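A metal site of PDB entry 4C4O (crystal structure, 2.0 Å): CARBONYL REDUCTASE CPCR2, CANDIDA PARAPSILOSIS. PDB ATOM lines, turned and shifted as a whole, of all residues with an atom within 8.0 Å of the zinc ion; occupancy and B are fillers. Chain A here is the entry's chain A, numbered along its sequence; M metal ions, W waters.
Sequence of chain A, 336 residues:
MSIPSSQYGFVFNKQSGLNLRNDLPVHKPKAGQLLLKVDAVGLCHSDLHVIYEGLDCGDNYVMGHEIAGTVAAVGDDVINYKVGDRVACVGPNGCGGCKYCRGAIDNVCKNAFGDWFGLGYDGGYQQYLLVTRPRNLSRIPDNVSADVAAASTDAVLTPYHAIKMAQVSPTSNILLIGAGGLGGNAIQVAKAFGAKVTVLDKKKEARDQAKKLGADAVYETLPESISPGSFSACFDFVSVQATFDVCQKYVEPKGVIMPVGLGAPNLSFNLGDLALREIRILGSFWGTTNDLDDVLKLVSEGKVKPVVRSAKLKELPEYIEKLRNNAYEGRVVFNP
The side-chain carboxylate of Asp 154 is in hydrogen-bond range of the side-chain hydroxyl of Thr 158 (2.9 Å).
The backbone NH (N) of Gly 42 lies within hydrogen-bond range of the backbone carbonyl oxygen (O) of Glu 66, 2.7 Å away.
The side-chain carboxylate (OD1) of Asp 47 lies within hydrogen-bond range of a ring nitrogen (ND1) of His 65 (3.2 Å).
Within 4 Å of the zinc ion: His 65, Glu 66 and Asp 154.
The nearest printed residue that does not touch the zinc ion is Ser 46 (4.9 Å).
The zinc ion is bound by the side-chain carboxylate of Asp 154 (2.0 Å), the side-chain carboxylate of Glu 66 (2.0 Å), a ring nitrogen (NE2) of His 65 (2.1 Å) and water W1 (2.4 Å).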
ATOM      1  N   GLY A  42       2.464  -3.280 -21.034  1.00  0.00           N
ATOM      2  CA  GLY A  42       3.623  -2.918 -20.196  1.00  0.00           C
ATOM      3  C   GLY A  42       3.348  -3.269 -18.764  1.00  0.00           C
ATOM      4  O   GLY A  42       2.206  -3.411 -18.386  1.00  0.00           O
ATOM      5  N   LEU A  43       4.401  -3.374 -17.956  1.00  0.00           N
ATOM      6  CA  LEU A  43       4.315  -3.634 -16.531  1.00  0.00           C
ATOM      7  C   LEU A  43       4.851  -2.413 -15.768  1.00  0.00           C
ATOM      8  O   LEU A  43       5.960  -1.976 -16.128  1.00  0.00           O
ATOM      9  CB  LEU A  43       5.164  -4.870 -16.192  1.00  0.00           C
ATOM     10  CG  LEU A  43       5.512  -5.186 -14.724  1.00  0.00           C
ATOM     11  CD1 LEU A  43       4.280  -5.329 -13.875  1.00  0.00           C
ATOM     12  CD2 LEU A  43       6.364  -6.461 -14.639  1.00  0.00           C
ATOM     13  N   HIS A  45       5.652  -0.066 -11.951  1.00  0.00           N
ATOM     14  CA  HIS A  45       5.744  -0.243 -10.473  1.00  0.00           C
ATOM     15  C   HIS A  45       4.358  -0.180  -9.852  1.00  0.00           C
ATOM     16  O   HIS A  45       4.145  -0.814  -8.825  1.00  0.00           O
ATOM     17  CB  HIS A  45       6.674   0.794  -9.799  1.00  0.00           C
ATOM     18  N   SER A  46       3.427   0.539 -10.490  1.00  0.00           N
ATOM     19  CA  SER A  46       2.058   0.652  -9.988  1.00  0.00           C
ATOM     20  C   SER A  46       1.294  -0.683  -9.913  1.00  0.00           C
ATOM     21  O   SER A  46       0.403  -0.854  -9.067  1.00  0.00           O
ATOM     22  CB  SER A  46       1.225   1.721 -10.776  1.00  0.00           C
ATOM     23  OG  SER A  46       1.737   3.019 -10.564  1.00  0.00           O
ATOM     24  N   ASP A  47       1.639  -1.660 -10.756  1.00  0.00           N
ATOM     25  CA  ASP A  47       1.012  -2.969 -10.621  1.00  0.00           C
ATOM     26  C   ASP A  47       1.408  -3.653  -9.290  1.00  0.00           C
ATOM     27  O   ASP A  47       0.574  -4.295  -8.642  1.00  0.00           O
ATOM     28  CB  ASP A  47       1.350  -3.861 -11.802  1.00  0.00           C
ATOM     29  CG  ASP A  47       0.753  -3.358 -13.088  1.00  0.00           C
ATOM     30  OD1 ASP A  47      -0.351  -2.772 -13.027  1.00  0.00           O
ATOM     31  OD2 ASP A  47       1.400  -3.508 -14.141  1.00  0.00           O
ATOM     32  N   GLY A  64      -2.937  -4.868 -16.242  1.00  0.00           N
ATOM     33  CA  GLY A  64      -2.167  -4.448 -17.407  1.00  0.00           C
ATOM     34  C   GLY A  64      -2.725  -3.119 -17.901  1.00  0.00           C
ATOM     35  O   GLY A  64      -3.722  -3.108 -18.626  1.00  0.00           O
ATOM     36  N   HIS A  65      -2.085  -2.001 -17.550  1.00  0.00           N
ATOM     37  CA  HIS A  65      -2.667  -0.658 -17.828  1.00  0.00           C
ATOM     38  C   HIS A  65      -1.887   0.124 -18.876  1.00  0.00           C
ATOM     39  O   HIS A  65      -2.140   1.319 -19.077  1.00  0.00           O
ATOM     40  CB  HIS A  65      -2.807   0.161 -16.547  1.00  0.00           C
ATOM     41  CG  HIS A  65      -1.504   0.539 -15.908  1.00  0.00           C
ATOM     42  ND1 HIS A  65      -0.954  -0.217 -14.891  1.00  0.00           N
ATOM     43  CD2 HIS A  65      -0.649   1.573 -16.106  1.00  0.00           C
ATOM     44  CE1 HIS A  65       0.177   0.342 -14.481  1.00  0.00           C
ATOM     45  NE2 HIS A  65       0.381   1.436 -15.204  1.00  0.00           N
ATOM     46  N   GLU A  66      -0.937  -0.532 -19.550  1.00  0.00           N
ATOM     47  CA  GLU A  66      -0.120   0.083 -20.588  1.00  0.00           C
ATOM     48  C   GLU A  66      -0.345  -0.760 -21.796  1.00  0.00           C
ATOM     49  O   GLU A  66       0.410  -1.735 -22.012  1.00  0.00           O
ATOM     50  CB  GLU A  66       1.368   0.076 -20.154  1.00  0.00           C
ATOM     51  CG  GLU A  66       1.560   0.836 -18.834  1.00  0.00           C
ATOM     52  CD  GLU A  66       2.987   0.918 -18.373  1.00  0.00           C
ATOM     53  OE1 GLU A  66       3.878   0.499 -19.140  1.00  0.00           O
ATOM     54  OE2 GLU A  66       3.218   1.451 -17.249  1.00  0.00           O
ATOM     55  N   LEU A 119      -6.868  -1.439 -13.967  1.00  0.00           N
ATOM     56  CA  LEU A 119      -6.846  -0.917 -12.588  1.00  0.00           C
ATOM     57  C   LEU A 119      -8.291  -0.630 -12.143  1.00  0.00           C
ATOM     58  O   LEU A 119      -8.666   0.511 -11.803  1.00  0.00           O
ATOM     59  CB  LEU A 119      -5.954   0.347 -12.469  1.00  0.00           C
ATOM     60  CG  LEU A 119      -4.416   0.202 -12.659  1.00  0.00           C
ATOM     61  CD1 LEU A 119      -3.696   1.531 -12.915  1.00  0.00           C
ATOM     62  CD2 LEU A 119      -3.829  -0.504 -11.452  1.00  0.00           C
ATOM     63  N   TYR A 125      -3.350  -7.614 -19.836  1.00  0.00           N
ATOM     64  CA  TYR A 125      -2.714  -8.929 -19.576  1.00  0.00           C
ATOM     65  C   TYR A 125      -3.629 -10.085 -20.050  1.00  0.00           C
ATOM     66  O   TYR A 125      -4.011 -10.942 -19.241  1.00  0.00           O
ATOM     67  CB  TYR A 125      -2.342  -9.122 -18.089  1.00  0.00           C
ATOM     68  CG  TYR A 125      -1.266  -8.209 -17.539  1.00  0.00           C
ATOM     69  CD1 TYR A 125      -0.204  -7.774 -18.327  1.00  0.00           C
ATOM     70  CD2 TYR A 125      -1.313  -7.809 -16.203  1.00  0.00           C
ATOM     71  CE1 TYR A 125       0.753  -6.925 -17.818  1.00  0.00           C
ATOM     72  CE2 TYR A 125      -0.328  -6.988 -15.671  1.00  0.00           C
ATOM     73  CZ  TYR A 125       0.700  -6.548 -16.485  1.00  0.00           C
ATOM     74  OH  TYR A 125       1.662  -5.718 -15.966  1.00  0.00           O
ATOM     75  N   ALA A 150       3.079   0.869 -26.290  1.00  0.00           N
ATOM     76  CA  ALA A 150       2.710   0.442 -24.965  1.00  0.00           C
ATOM     77  C   ALA A 150       3.561   1.132 -23.905  1.00  0.00           C
ATOM     78  O   ALA A 150       3.044   1.542 -22.874  1.00  0.00           O
ATOM     79  CB  ALA A 150       2.795  -1.112 -24.828  1.00  0.00           C
ATOM     80  N   ALA A 151       4.873   1.177 -24.118  1.00  0.00           N
ATOM     81  CA  ALA A 151       5.757   1.796 -23.129  1.00  0.00           C
ATOM     82  C   ALA A 151       5.597   3.317 -23.021  1.00  0.00           C
ATOM     83  O   ALA A 151       6.052   3.897 -22.081  1.00  0.00           O
ATOM     84  CB  ALA A 151       7.205   1.503 -23.479  1.00  0.00           C
ATOM     85  N   THR A 153       2.476   4.736 -22.889  1.00  0.00           N
ATOM     86  CA  THR A 153       1.125   5.028 -22.427  1.00  0.00           C
ATOM     87  C   THR A 153       1.100   5.514 -20.986  1.00  0.00           C
ATOM     88  O   THR A 153       0.076   6.011 -20.508  1.00  0.00           O
ATOM     89  CB  THR A 153       0.179   3.803 -22.518  1.00  0.00           C
ATOM     90  OG1 THR A 153       0.830   2.661 -21.950  1.00  0.00           O
ATOM     91  CG2 THR A 153      -0.128   3.491 -23.954  1.00  0.00           C
ATOM     92  N   ASP A 154       2.218   5.362 -20.278  1.00  0.00           N
ATOM     93  CA  ASP A 154       2.337   5.831 -18.922  1.00  0.00           C
ATOM     94  C   ASP A 154       3.744   6.488 -18.710  1.00  0.00           C
ATOM     95  O   ASP A 154       3.830   7.632 -18.267  1.00  0.00           O
ATOM     96  CB  ASP A 154       2.096   4.641 -17.983  1.00  0.00           C
ATOM     97  CG  ASP A 154       2.147   4.994 -16.505  1.00  0.00           C
ATOM     98  OD1 ASP A 154       2.076   6.211 -16.160  1.00  0.00           O
ATOM     99  OD2 ASP A 154       2.213   4.012 -15.694  1.00  0.00           O
ATOM    100  N   ALA A 155       4.820   5.754 -18.994  1.00  0.00           N
ATOM    101  CA  ALA A 155       6.199   6.280 -18.756  1.00  0.00           C
ATOM    102  C   ALA A 155       6.528   7.584 -19.522  1.00  0.00           C
ATOM    103  O   ALA A 155       7.333   8.385 -19.061  1.00  0.00           O
ATOM    104  CB  ALA A 155       7.224   5.222 -19.109  1.00  0.00           C
ATOM    105  N   THR A 158       2.808  10.352 -18.721  1.00  0.00           N
ATOM    106  CA  THR A 158       2.777  11.032 -17.479  1.00  0.00           C
ATOM    107  C   THR A 158       3.680  12.281 -17.373  1.00  0.00           C
ATOM    108  O   THR A 158       3.180  13.372 -17.025  1.00  0.00           O
ATOM    109  CB  THR A 158       2.960  10.019 -16.292  1.00  0.00           C
ATOM    110  OG1 THR A 158       1.843   9.118 -16.298  1.00  0.00           O
ATOM    111  CG2 THR A 158       2.953  10.728 -14.985  1.00  0.00           C
ATOM    112  N   LEU A 182      10.264   7.613 -15.056  1.00  0.00           N
ATOM    113  CA  LEU A 182       9.547   8.827 -15.507  1.00  0.00           C
ATOM    114  C   LEU A 182      10.542   9.965 -15.752  1.00  0.00           C
ATOM    115  O   LEU A 182      10.466  10.621 -16.781  1.00  0.00           O
ATOM    116  CB  LEU A 182       8.505   9.259 -14.481  1.00  0.00           C
ATOM    117  CG  LEU A 182       7.062   8.782 -14.757  1.00  0.00           C
ATOM    118  CD1 LEU A 182       6.957   7.269 -14.845  1.00  0.00           C
ATOM    119  CD2 LEU A 182       6.084   9.328 -13.729  1.00  0.00           C
ATOM    120  N   TRP A 286      -1.385  11.201 -14.516  1.00  0.00           N
ATOM    121  CA  TRP A 286      -1.397  10.406 -15.755  1.00  0.00           C
ATOM    122  C   TRP A 286      -1.414  11.312 -16.971  1.00  0.00           C
ATOM    123  O   TRP A 286      -0.564  12.219 -17.045  1.00  0.00           O
ATOM    124  CB  TRP A 286      -2.523   9.400 -15.721  1.00  0.00           C
ATOM    125  CG  TRP A 286      -2.249   8.086 -16.410  1.00  0.00           C
ATOM    126  CD1 TRP A 286      -1.385   7.874 -17.448  1.00  0.00           C
ATOM    127  CD2 TRP A 286      -2.871   6.807 -16.130  1.00  0.00           C
ATOM    128  NE1 TRP A 286      -1.412   6.543 -17.814  1.00  0.00           N
ATOM    129  CE2 TRP A 286      -2.317   5.871 -17.045  1.00  0.00           C
ATOM    130  CE3 TRP A 286      -3.793   6.343 -15.172  1.00  0.00           C
ATOM    131  CZ2 TRP A 286      -2.674   4.487 -17.042  1.00  0.00           C
ATOM    132  CZ3 TRP A 286      -4.180   4.985 -15.206  1.00  0.00           C
ATOM    133  CH2 TRP A 286      -3.590   4.076 -16.122  1.00  0.00           C
HETATM  134 ZN    ZN M   1       2.344   2.008 -15.513  1.00  0.00          ZN
HETATM  135  O   HOH W   1       3.662   1.352 -13.585  1.00  0.00           O
